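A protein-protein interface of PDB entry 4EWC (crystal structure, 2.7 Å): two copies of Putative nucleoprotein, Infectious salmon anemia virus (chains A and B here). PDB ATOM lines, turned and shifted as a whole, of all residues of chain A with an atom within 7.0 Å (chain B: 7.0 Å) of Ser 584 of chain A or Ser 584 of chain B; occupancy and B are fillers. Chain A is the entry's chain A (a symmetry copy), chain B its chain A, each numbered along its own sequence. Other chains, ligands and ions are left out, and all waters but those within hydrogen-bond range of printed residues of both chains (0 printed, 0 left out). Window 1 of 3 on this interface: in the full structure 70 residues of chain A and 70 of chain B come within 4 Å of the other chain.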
ATOM      1  N   SER A 456     -30.465 -28.525  14.323  1.00  0.00           N
ATOM      2  CA  SER A 456     -30.563 -27.228  14.965  1.00  0.00           C
ATOM      3  C   SER A 456     -31.682 -27.201  16.009  1.00  0.00           C
ATOM      4  O   SER A 456     -32.790 -27.709  15.768  1.00  0.00           O
ATOM      5  CB  SER A 456     -30.822 -26.145  13.904  1.00  0.00           C
ATOM      6  OG  SER A 456     -31.388 -24.980  14.483  1.00  0.00           O
ATOM      7  N   ALA A 457     -31.385 -26.624  17.170  1.00  0.00           N
ATOM      8  CA  ALA A 457     -32.385 -26.470  18.223  1.00  0.00           C
ATOM      9  C   ALA A 457     -33.515 -25.535  17.796  1.00  0.00           C
ATOM     10  O   ALA A 457     -34.675 -25.793  18.110  1.00  0.00           O
ATOM     11  CB  ALA A 457     -31.741 -25.966  19.512  1.00  0.00           C
ATOM     12  N   ASP A 458     -33.169 -24.455  17.097  1.00  0.00           N
ATOM     13  CA  ASP A 458     -34.174 -23.538  16.576  1.00  0.00           C
ATOM     14  C   ASP A 458     -35.187 -24.299  15.735  1.00  0.00           C
ATOM     15  O   ASP A 458     -36.395 -24.084  15.853  1.00  0.00           O
ATOM     16  CB  ASP A 458     -33.545 -22.461  15.719  1.00  0.00           C
ATOM     17  CG  ASP A 458     -32.611 -21.563  16.498  1.00  0.00           C
ATOM     18  OD1 ASP A 458     -33.136 -20.706  17.244  1.00  0.00           O
ATOM     19  OD2 ASP A 458     -31.362 -21.697  16.346  1.00  0.00           O
ATOM     20  N   ARG A 469     -35.472 -27.238  24.371  1.00  0.00           N
ATOM     21  CA  ARG A 469     -34.377 -26.906  23.468  1.00  0.00           C
ATOM     22  C   ARG A 469     -32.987 -27.275  24.030  1.00  0.00           C
ATOM     23  O   ARG A 469     -31.985 -27.336  23.295  1.00  0.00           O
ATOM     24  CB  ARG A 469     -34.476 -25.426  23.085  1.00  0.00           C
ATOM     25  CG  ARG A 469     -33.185 -24.661  22.978  1.00  0.00           C
ATOM     26  CD  ARG A 469     -33.421 -23.160  22.828  1.00  0.00           C
ATOM     27  NE  ARG A 469     -33.857 -22.762  21.489  1.00  0.00           N
ATOM     28  CZ  ARG A 469     -33.059 -22.194  20.587  1.00  0.00           C
ATOM     29  NH1 ARG A 469     -31.784 -21.965  20.878  1.00  0.00           N
ATOM     30  NH2 ARG A 469     -33.537 -21.846  19.399  1.00  0.00           N
ATOM     31  N   TYR A 470     -32.927 -27.545  25.338  1.00  0.00           N
ATOM     32  CA  TYR A 470     -31.679 -28.006  25.965  1.00  0.00           C
ATOM     33  C   TYR A 470     -31.775 -29.402  26.578  1.00  0.00           C
ATOM     34  O   TYR A 470     -32.628 -29.677  27.410  1.00  0.00           O
ATOM     35  CB  TYR A 470     -31.147 -27.010  26.999  1.00  0.00           C
ATOM     36  CG  TYR A 470     -30.973 -25.610  26.472  1.00  0.00           C
ATOM     37  CD1 TYR A 470     -29.856 -25.261  25.741  1.00  0.00           C
ATOM     38  CD2 TYR A 470     -31.935 -24.634  26.715  1.00  0.00           C
ATOM     39  CE1 TYR A 470     -29.695 -23.981  25.259  1.00  0.00           C
ATOM     40  CE2 TYR A 470     -31.779 -23.356  26.242  1.00  0.00           C
ATOM     41  CZ  TYR A 470     -30.652 -23.037  25.510  1.00  0.00           C
ATOM     42  OH  TYR A 470     -30.494 -21.769  25.029  1.00  0.00           O
ATOM     43  N   VAL A 518     -25.279  -9.104  19.907  1.00  0.00           N
ATOM     44  CA  VAL A 518     -26.293  -8.817  20.895  1.00  0.00           C
ATOM     45  C   VAL A 518     -25.596  -8.536  22.208  1.00  0.00           C
ATOM     46  O   VAL A 518     -24.389  -8.718  22.326  1.00  0.00           O
ATOM     47  CB  VAL A 518     -27.309  -9.956  21.053  1.00  0.00           C
ATOM     48  CG1 VAL A 518     -28.116 -10.068  19.795  1.00  0.00           C
ATOM     49  CG2 VAL A 518     -26.603 -11.274  21.339  1.00  0.00           C
ATOM     50  N   VAL A 527     -22.376 -10.939  22.627  1.00  0.00           N
ATOM     51  CA  VAL A 527     -22.119 -12.088  21.775  1.00  0.00           C
ATOM     52  C   VAL A 527     -22.214 -11.583  20.356  1.00  0.00           C
ATOM     53  O   VAL A 527     -23.083 -10.779  20.025  1.00  0.00           O
ATOM     54  CB  VAL A 527     -23.091 -13.270  22.030  1.00  0.00           C
ATOM     55  CG1 VAL A 527     -22.898 -14.376  20.984  1.00  0.00           C
ATOM     56  CG2 VAL A 527     -22.865 -13.830  23.396  1.00  0.00           C
ATOM     57  N   PHE A 528     -21.308 -12.036  19.513  1.00  0.00           N
ATOM     58  CA  PHE A 528     -21.181 -11.446  18.190  1.00  0.00           C
ATOM     59  C   PHE A 528     -20.820 -12.483  17.118  1.00  0.00           C
ATOM     60  O   PHE A 528     -20.323 -13.562  17.438  1.00  0.00           O
ATOM     61  CB  PHE A 528     -20.128 -10.339  18.262  1.00  0.00           C
ATOM     62  CG  PHE A 528     -18.817 -10.805  18.787  1.00  0.00           C
ATOM     63  CD1 PHE A 528     -17.855 -11.326  17.930  1.00  0.00           C
ATOM     64  CD2 PHE A 528     -18.539 -10.737  20.146  1.00  0.00           C
ATOM     65  CE1 PHE A 528     -16.641 -11.769  18.425  1.00  0.00           C
ATOM     66  CE2 PHE A 528     -17.329 -11.175  20.639  1.00  0.00           C
ATOM     67  CZ  PHE A 528     -16.385 -11.692  19.780  1.00  0.00           C
ATOM     68  N   ASN A 529     -21.096 -12.154  15.856  1.00  0.00           N
ATOM     69  CA  ASN A 529     -20.775 -13.028  14.725  1.00  0.00           C
ATOM     70  C   ASN A 529     -19.302 -12.859  14.313  1.00  0.00           C
ATOM     71  O   ASN A 529     -18.932 -11.859  13.682  1.00  0.00           O
ATOM     72  CB  ASN A 529     -21.680 -12.694  13.556  1.00  0.00           C
ATOM     73  CG  ASN A 529     -21.439 -13.573  12.343  1.00  0.00           C
ATOM     74  OD1 ASN A 529     -20.313 -13.698  11.856  1.00  0.00           O
ATOM     75  ND2 ASN A 529     -22.516 -14.171  11.826  1.00  0.00           N
ATOM     76  N   VAL A 568     -27.565 -17.631   8.719  1.00  0.00           N
ATOM     77  CA  VAL A 568     -28.263 -18.600   7.882  1.00  0.00           C
ATOM     78  C   VAL A 568     -29.741 -18.665   8.222  1.00  0.00           C
ATOM     79  O   VAL A 568     -30.122 -18.941   9.365  1.00  0.00           O
ATOM     80  CB  VAL A 568     -27.687 -20.004   8.081  1.00  0.00           C
ATOM     81  CG1 VAL A 568     -28.394 -20.993   7.170  1.00  0.00           C
ATOM     82  CG2 VAL A 568     -26.179 -19.997   7.849  1.00  0.00           C
ATOM     83  N   ILE A 581     -36.991 -18.424   9.916  1.00  0.00           N
ATOM     84  CA  ILE A 581     -36.225 -18.440  11.169  1.00  0.00           C
ATOM     85  C   ILE A 581     -34.745 -18.461  10.839  1.00  0.00           C
ATOM     86  O   ILE A 581     -34.367 -18.788   9.713  1.00  0.00           O
ATOM     87  CB  ILE A 581     -36.536 -19.665  12.075  1.00  0.00           C
ATOM     88  CG1 ILE A 581     -36.025 -20.961  11.451  1.00  0.00           C
ATOM     89  CG2 ILE A 581     -38.026 -19.742  12.416  1.00  0.00           C
ATOM     90  CD1 ILE A 581     -35.869 -22.091  12.438  1.00  0.00           C
ATOM     91  N   VAL A 582     -33.916 -18.112  11.821  1.00  0.00           N
ATOM     92  CA  VAL A 582     -32.457 -18.196  11.691  1.00  0.00           C
ATOM     93  C   VAL A 582     -31.910 -19.456  12.357  1.00  0.00           C
ATOM     94  O   VAL A 582     -32.186 -19.731  13.521  1.00  0.00           O
ATOM     95  CB  VAL A 582     -31.744 -16.988  12.363  1.00  0.00           C
ATOM     96  CG1 VAL A 582     -30.262 -17.294  12.578  1.00  0.00           C
ATOM     97  CG2 VAL A 582     -31.924 -15.725  11.554  1.00  0.00           C
ATOM     98  N   ILE A 583     -31.120 -20.224  11.627  1.00  0.00           N
ATOM     99  CA  ILE A 583     -30.403 -21.324  12.268  1.00  0.00           C
ATOM    100  C   ILE A 583     -29.176 -20.722  12.969  1.00  0.00           C
ATOM    101  O   ILE A 583     -28.205 -20.312  12.318  1.00  0.00           O
ATOM    102  CB  ILE A 583     -30.000 -22.413  11.243  1.00  0.00           C
ATOM    103  CG1 ILE A 583     -31.233 -22.893  10.498  1.00  0.00           C
ATOM    104  CG2 ILE A 583     -29.331 -23.589  11.914  1.00  0.00           C
ATOM    105  CD1 ILE A 583     -30.910 -23.664   9.234  1.00  0.00           C
ATOM    106  N   SER A 584     -29.250 -20.653  14.295  1.00  0.00           N
ATOM    107  CA  SER A 584     -28.256 -19.950  15.102  1.00  0.00           C
ATOM    108  C   SER A 584     -26.939 -20.689  15.217  1.00  0.00           C
ATOM    109  O   SER A 584     -25.882 -20.071  15.346  1.00  0.00           O
ATOM    110  CB  SER A 584     -28.788 -19.701  16.517  1.00  0.00           C
ATOM    111  OG  SER A 584     -29.202 -20.912  17.109  1.00  0.00           O
ATOM    112  N   GLY A 585     -27.012 -22.009  15.182  1.00  0.00           N
ATOM    113  CA  GLY A 585     -25.853 -22.839  15.395  1.00  0.00           C
ATOM    114  C   GLY A 585     -25.972 -23.553  16.731  1.00  0.00           C
ATOM    115  O   GLY A 585     -25.295 -24.546  16.968  1.00  0.00           O
ATOM    116  N   VAL A 586     -26.829 -23.049  17.613  1.00  0.00           N
ATOM    117  CA  VAL A 586     -27.073 -23.739  18.870  1.00  0.00           C
ATOM    118  C   VAL A 586     -27.834 -25.022  18.573  1.00  0.00           C
ATOM    119  O   VAL A 586     -28.702 -25.057  17.692  1.00  0.00           O
ATOM    120  CB  VAL A 586     -27.884 -22.879  19.890  1.00  0.00           C
ATOM    121  CG1 VAL A 586     -28.209 -23.692  21.142  1.00  0.00           C
ATOM    122  CG2 VAL A 586     -27.099 -21.661  20.274  1.00  0.00           C
ATOM    123  N   GLY A 587     -27.500 -26.087  19.286  1.00  0.00           N
ATOM    124  CA  GLY A 587     -28.269 -27.289  19.154  1.00  0.00           C
ATOM    125  C   GLY A 587     -28.633 -27.832  20.508  1.00  0.00           C
ATOM    126  O   GLY A 587     -28.461 -27.187  21.553  1.00  0.00           O
ATOM    127  N   SER B 456     -30.049 -10.035  23.496  1.00  0.00           N
ATOM    128  CA  SER B 456     -30.170 -11.367  22.933  1.00  0.00           C
ATOM    129  C   SER B 456     -31.633 -11.804  22.833  1.00  0.00           C
ATOM    130  O   SER B 456     -32.424 -11.598  23.768  1.00  0.00           O
ATOM    131  CB  SER B 456     -29.392 -12.367  23.804  1.00  0.00           C
ATOM    132  OG  SER B 456     -29.848 -13.694  23.599  1.00  0.00           O
ATOM    133  N   ALA B 457     -31.992 -12.391  21.695  1.00  0.00           N
ATOM    134  CA  ALA B 457     -33.340 -12.918  21.500  1.00  0.00           C
ATOM    135  C   ALA B 457     -33.634 -14.079  22.448  1.00  0.00           C
ATOM    136  O   ALA B 457     -34.745 -14.182  22.965  1.00  0.00           O
ATOM    137  CB  ALA B 457     -33.547 -13.353  20.052  1.00  0.00           C
ATOM    138  N   ASP B 458     -32.646 -14.947  22.659  1.00  0.00           N
ATOM    139  CA  ASP B 458     -32.796 -16.047  23.602  1.00  0.00           C
ATOM    140  C   ASP B 458     -33.208 -15.514  24.965  1.00  0.00           C
ATOM    141  O   ASP B 458     -34.100 -16.062  25.614  1.00  0.00           O
ATOM    142  CB  ASP B 458     -31.502 -16.819  23.757  1.00  0.00           C
ATOM    143  CG  ASP B 458     -31.071 -17.500  22.478  1.00  0.00           C
ATOM    144  OD1 ASP B 458     -31.687 -18.538  22.149  1.00  0.00           O
ATOM    145  OD2 ASP B 458     -30.104 -17.014  21.820  1.00  0.00           O
ATOM    146  N   ARG B 469     -39.670 -13.646  18.795  1.00  0.00           N
ATOM    147  CA  ARG B 469     -38.214 -13.573  18.766  1.00  0.00           C
ATOM    148  C   ARG B 469     -37.662 -12.895  17.493  1.00  0.00           C
ATOM    149  O   ARG B 469     -36.487 -12.488  17.432  1.00  0.00           O
ATOM    150  CB  ARG B 469     -37.639 -14.977  18.975  1.00  0.00           C
ATOM    151  CG  ARG B 469     -36.425 -15.344  18.166  1.00  0.00           C
ATOM    152  CD  ARG B 469     -36.090 -16.829  18.279  1.00  0.00           C
ATOM    153  NE  ARG B 469     -35.452 -17.196  19.545  1.00  0.00           N
ATOM    154  CZ  ARG B 469     -34.148 -17.429  19.678  1.00  0.00           C
ATOM    155  NH1 ARG B 469     -33.343 -17.328  18.627  1.00  0.00           N
ATOM    156  NH2 ARG B 469     -33.650 -17.774  20.859  1.00  0.00           N
ATOM    157  N   TYR B 470     -38.517 -12.752  16.476  1.00  0.00           N
ATOM    158  CA  TYR B 470     -38.134 -12.032  15.253  1.00  0.00           C
ATOM    159  C   TYR B 470     -38.973 -10.784  14.982  1.00  0.00           C
ATOM    160  O   TYR B 470     -40.193 -10.838  14.907  1.00  0.00           O
ATOM    161  CB  TYR B 470     -38.127 -12.942  14.022  1.00  0.00           C
ATOM    162  CG  TYR B 470     -37.284 -14.181  14.177  1.00  0.00           C
ATOM    163  CD1 TYR B 470     -35.917 -14.135  13.999  1.00  0.00           C
ATOM    164  CD2 TYR B 470     -37.868 -15.402  14.499  1.00  0.00           C
ATOM    165  CE1 TYR B 470     -35.145 -15.267  14.140  1.00  0.00           C
ATOM    166  CE2 TYR B 470     -37.106 -16.534  14.636  1.00  0.00           C
ATOM    167  CZ  TYR B 470     -35.739 -16.457  14.457  1.00  0.00           C
ATOM    168  OH  TYR B 470     -34.972 -17.578  14.600  1.00  0.00           O
ATOM    169  N   VAL B 518     -24.484 -27.748  13.980  1.00  0.00           N
ATOM    170  CA  VAL B 518     -25.765 -28.400  13.831  1.00  0.00           C
ATOM    171  C   VAL B 518     -26.010 -28.609  12.352  1.00  0.00           C
ATOM    172  O   VAL B 518     -25.259 -28.115  11.519  1.00  0.00           O
ATOM    173  CB  VAL B 518     -26.913 -27.605  14.465  1.00  0.00           C
ATOM    174  CG1 VAL B 518     -26.736 -27.593  15.953  1.00  0.00           C
ATOM    175  CG2 VAL B 518     -26.944 -26.179  13.932  1.00  0.00           C
ATOM    176  N   VAL B 527     -24.597 -25.469  10.240  1.00  0.00           N
ATOM    177  CA  VAL B 527     -24.188 -24.215  10.848  1.00  0.00           C
ATOM    178  C   VAL B 527     -23.222 -24.582  11.949  1.00  0.00           C
ATOM    179  O   VAL B 527     -23.423 -25.556  12.672  1.00  0.00           O
ATOM    180  CB  VAL B 527     -25.378 -23.376  11.384  1.00  0.00           C
ATOM    181  CG1 VAL B 527     -24.881 -22.160  12.177  1.00  0.00           C
ATOM    182  CG2 VAL B 527     -26.229 -22.915  10.246  1.00  0.00           C
ATOM    183  N   PHE B 528     -22.157 -23.816  12.071  1.00  0.00           N
ATOM    184  CA  PHE B 528     -21.069 -24.212  12.950  1.00  0.00           C
ATOM    185  C   PHE B 528     -20.415 -23.014  13.651  1.00  0.00           C
ATOM    186  O   PHE B 528     -20.552 -21.878  13.199  1.00  0.00           O
ATOM    187  CB  PHE B 528     -20.046 -24.990  12.119  1.00  0.00           C
ATOM    188  CG  PHE B 528     -19.554 -24.237  10.934  1.00  0.00           C
ATOM    189  CD1 PHE B 528     -18.458 -23.389  11.040  1.00  0.00           C
ATOM    190  CD2 PHE B 528     -20.191 -24.362   9.707  1.00  0.00           C
ATOM    191  CE1 PHE B 528     -18.010 -22.682   9.937  1.00  0.00           C
ATOM    192  CE2 PHE B 528     -19.744 -23.661   8.608  1.00  0.00           C
ATOM    193  CZ  PHE B 528     -18.659 -22.821   8.725  1.00  0.00           C
ATOM    194  N   ASN B 529     -19.728 -23.278  14.762  1.00  0.00           N
ATOM    195  CA  ASN B 529     -19.021 -22.240  15.519  1.00  0.00           C
ATOM    196  C   ASN B 529     -17.646 -21.957  14.889  1.00  0.00           C
ATOM    197  O   ASN B 529     -16.705 -22.748  15.040  1.00  0.00           O
ATOM    198  CB  ASN B 529     -18.849 -22.691  16.955  1.00  0.00           C
ATOM    199  CG  ASN B 529     -18.149 -21.663  17.824  1.00  0.00           C
ATOM    200  OD1 ASN B 529     -17.059 -21.185  17.501  1.00  0.00           O
ATOM    201  ND2 ASN B 529     -18.769 -21.334  18.962  1.00  0.00           N
ATOM    202  N   VAL B 568     -21.422 -19.098  24.885  1.00  0.00           N
ATOM    203  CA  VAL B 568     -21.665 -18.278  26.066  1.00  0.00           C
ATOM    204  C   VAL B 568     -22.971 -18.656  26.743  1.00  0.00           C
ATOM    205  O   VAL B 568     -24.044 -18.610  26.132  1.00  0.00           O
ATOM    206  CB  VAL B 568     -21.758 -16.798  25.690  1.00  0.00           C
ATOM    207  CG1 VAL B 568     -21.968 -15.954  26.936  1.00  0.00           C
ATOM    208  CG2 VAL B 568     -20.516 -16.368  24.916  1.00  0.00           C
ATOM    209  N   ILE B 581     -29.235 -21.043  29.991  1.00  0.00           N
ATOM    210  CA  ILE B 581     -29.474 -20.944  28.545  1.00  0.00           C
ATOM    211  C   ILE B 581     -28.198 -20.485  27.867  1.00  0.00           C
ATOM    212  O   ILE B 581     -27.302 -19.956  28.527  1.00  0.00           O
ATOM    213  CB  ILE B 581     -30.607 -19.948  28.167  1.00  0.00           C
ATOM    214  CG1 ILE B 581     -30.198 -18.506  28.454  1.00  0.00           C
ATOM    215  CG2 ILE B 581     -31.925 -20.318  28.853  1.00  0.00           C
ATOM    216  CD1 ILE B 581     -31.018 -17.482  27.710  1.00  0.00           C
ATOM    217  N   VAL B 582     -28.120 -20.689  26.553  1.00  0.00           N
ATOM    218  CA  VAL B 582     -27.003 -20.197  25.741  1.00  0.00           C
ATOM    219  C   VAL B 582     -27.370 -18.908  25.010  1.00  0.00           C
ATOM    220  O   VAL B 582     -28.381 -18.837  24.316  1.00  0.00           O
ATOM    221  CB  VAL B 582     -26.578 -21.224  24.653  1.00  0.00           C
ATOM    222  CG1 VAL B 582     -25.722 -20.546  23.583  1.00  0.00           C
ATOM    223  CG2 VAL B 582     -25.852 -22.400  25.263  1.00  0.00           C
ATOM    224  N   ILE B 583     -26.548 -17.884  25.150  1.00  0.00           N
ATOM    225  CA  ILE B 583     -26.733 -16.700  24.315  1.00  0.00           C
ATOM    226  C   ILE B 583     -26.120 -17.009  22.940  1.00  0.00           C
ATOM    227  O   ILE B 583     -24.892 -17.070  22.788  1.00  0.00           O
ATOM    228  CB  ILE B 583     -26.093 -15.444  24.958  1.00  0.00           C
ATOM    229  CG1 ILE B 583     -26.649 -15.249  26.358  1.00  0.00           C
ATOM    230  CG2 ILE B 583     -26.352 -14.204  24.137  1.00  0.00           C
ATOM    231  CD1 ILE B 583     -25.828 -14.296  27.203  1.00  0.00           C
ATOM    232  N   SER B 584     -26.991 -17.228  21.961  1.00  0.00           N
ATOM    233  CA  SER B 584     -26.587 -17.709  20.642  1.00  0.00           C
ATOM    234  C   SER B 584     -25.906 -16.653  19.797  1.00  0.00           C
ATOM    235  O   SER B 584     -25.051 -16.966  18.968  1.00  0.00           O
ATOM    236  CB  SER B 584     -27.797 -18.234  19.865  1.00  0.00           C
ATOM    237  OG  SER B 584     -28.803 -17.250  19.792  1.00  0.00           O
ATOM    238  N   GLY B 585     -26.299 -15.407  20.002  1.00  0.00           N
ATOM    239  CA  GLY B 585     -25.819 -14.316  19.190  1.00  0.00           C
ATOM    240  C   GLY B 585     -26.945 -13.800  18.309  1.00  0.00           C
ATOM    241  O   GLY B 585     -26.875 -12.688  17.799  1.00  0.00           O
ATOM    242  N   VAL B 586     -27.985 -14.606  18.121  1.00  0.00           N
ATOM    243  CA  VAL B 586     -29.144 -14.139  17.377  1.00  0.00           C
ATOM    244  C   VAL B 586     -29.861 -13.090  18.214  1.00  0.00           C
ATOM    245  O   VAL B 586     -29.945 -13.206  19.443  1.00  0.00           O
ATOM    246  CB  VAL B 586     -30.140 -15.286  17.018  1.00  0.00           C
ATOM    247  CG1 VAL B 586     -31.389 -14.722  16.341  1.00  0.00           C
ATOM    248  CG2 VAL B 586     -29.479 -16.274  16.105  1.00  0.00           C
ATOM    249  N   GLY B 587     -30.360 -12.052  17.562  1.00  0.00           N
ATOM    250  CA  GLY B 587     -31.165 -11.099  18.269  1.00  0.00           C
ATOM    251  C   GLY B 587     -32.432 -10.815  17.511  1.00  0.00           C
ATOM    252  O   GLY B 587     -32.789 -11.491  16.534  1.00  0.00           O
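Ala 457 of chain A touches none of the printed residues of chain B.
Printed residues of chain B within 4 Å of Val 527 of chain A: Val 568 (3.8 Å), Ile 583 (3.6 Å), Ser 584 (3.9 Å) and Gly 585 (3.4 Å).
Printed residues of chain B within 4 Å of Val 582 of chain A: Tyr 470 (3.0 Å) and Val 586 (3.8 Å).
Of chain B, only Val 527, Ser 584 and Val 586 come within 4 Å of Ser 584 of chain A.
Of the printed residues of chain A, Tyr 470 of chain B touches Ile 581 and Val 582.
Phe 528 of chain B touches none of the printed residues of chain A.
Printed residues of chain A within 4 Å of Val 568 of chain B: Val 527.
Ser 584 of chain B touches three residues of chain A.
Printed residues of chain A within 4 Å of Gly 585 of chain B: Val 518 and Val 527.
The nearest printed residue of chain B that does not touch Tyr 470 of chain A is Asp 458 of chain B (4.5 Å).
The guanidinium group of Arg 469 of chain B is in salt-bridge range of the side-chain carboxylate of Asp 458 of chain A (3.7 Å).
The side-chain hydroxyl of Tyr 470 of chain B sits at hydrogen-bond distance from the backbone NH of Val 582 of chain A.
N of Val 582 of chain B lies within hydrogen-bond range of OH of Tyr 470 of chain A (3.0 Å).
The guanidinium group of Arg 469 of chain A lies within salt-bridge range of the side-chain carboxylate of Asp 458 of chain B (3.7 Å).
Tyr 470 of chain A touches Ile 581 of chain B, and with the chains exchanged Ile 581 of chain A touches Tyr 470 of chain B.
Val 527 of chain A touches Ile 583 of chain B, and with the chains exchanged Ile 583 of chain A touches Val 527 of chain B.
Ser 584 of chain B touches its own counterpart, Ser 584 of chain A.
Ser 584 of chain A touches Val 586 of chain B, and with the chains exchanged Val 586 of chain A touches Ser 584 of chain B.
Positions printed for both chains: 456, 457, 458, 469, 470, 518, 527, 528, 529, 568, 581, 582, 583, 584, 585, 586 and 587.
Of the 27 pairs that touch across the chains among the printed residues, 27 have their exchanged pair printed and touching as well.
Printed residues of chain A that touch a printed residue of chain B: Ser 456, Asp 458, Arg 469, Tyr 470, Val 518, Val 527, Val 568, Ile 581, Val 582, Ile 583, Ser 584, Gly 585, Val 586 and Gly 587.
Hydrophobic or aromatic side chains of chain A within 4 Å of the printed part of chain B: Tyr 470, Val 518, Val 527, Val 568, Ile 581, Val 582, Ile 583 and Val 586.
Of the 17 printed residues of chain B, 14 touch a printed residue of chain A.
Hydrophobic or aromatic side chains of chain B that line the printed part of chain A: Tyr 470, Val 518, Val 527, Val 568, Ile 581, Val 582, Ile 583 and Val 586.
Along chain B the printed residues that touch a printed residue of chain A span positions 456 to 587.
O of Val 527 of chain A is in hydrogen-bond range of N of Val 518 of chain A, at 2.8 Å.
N of Val 586 of chain B is in hydrogen-bond range of OG of Ser 584 of chain B.
The side-chain hydroxyl (OG) of Ser 584 of chain A lies within hydrogen-bond range of the side-chain carboxylate (OD2) of Asp 458 of chain A, at 2.4 Å.
N of Val 518 of chain B sits at hydrogen-bond distance from O of Val 527 of chain B (2.8 Å).
OG of Ser 584 of chain A is in hydrogen-bond range of N of Val 586 of chain A (3.2 Å).
The side-chain carboxylate (OD1) of Asp 458 of chain A is in salt-bridge range of the guanidinium group (NH2) of Arg 469 of chain A (2.5 Å).
Val 527 of chain A touches Val 568 of chain B.
Val 527 of chain A touches Ile 583 of chain B.
CG1 of Val 527 of chain A touches O of Ser 584 of chain B, 3.9 Å away.
CG2 of Val 568 of chain A touches CG2 of Val 527 of chain B, 3.8 Å away.
CG2 of Val 586 of chain B touches CG1 of Val 582 of chain A (3.8 Å).
Val 527 of chain B touches Ser 584 of chain A.
CB of Ser 584 of chain A touches CG2 of Val 586 of chain B (3.5 Å).
CG1 of Val 518 of chain B touches O of Gly 585 of chain A (3.5 Å).
Val 582 of chain B touches Val 586 of chain A (CG1 to CG2, 3.8 Å).
CG1 of Val 518 of chain B touches CA of Gly 587 of chain A (3.6 Å).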
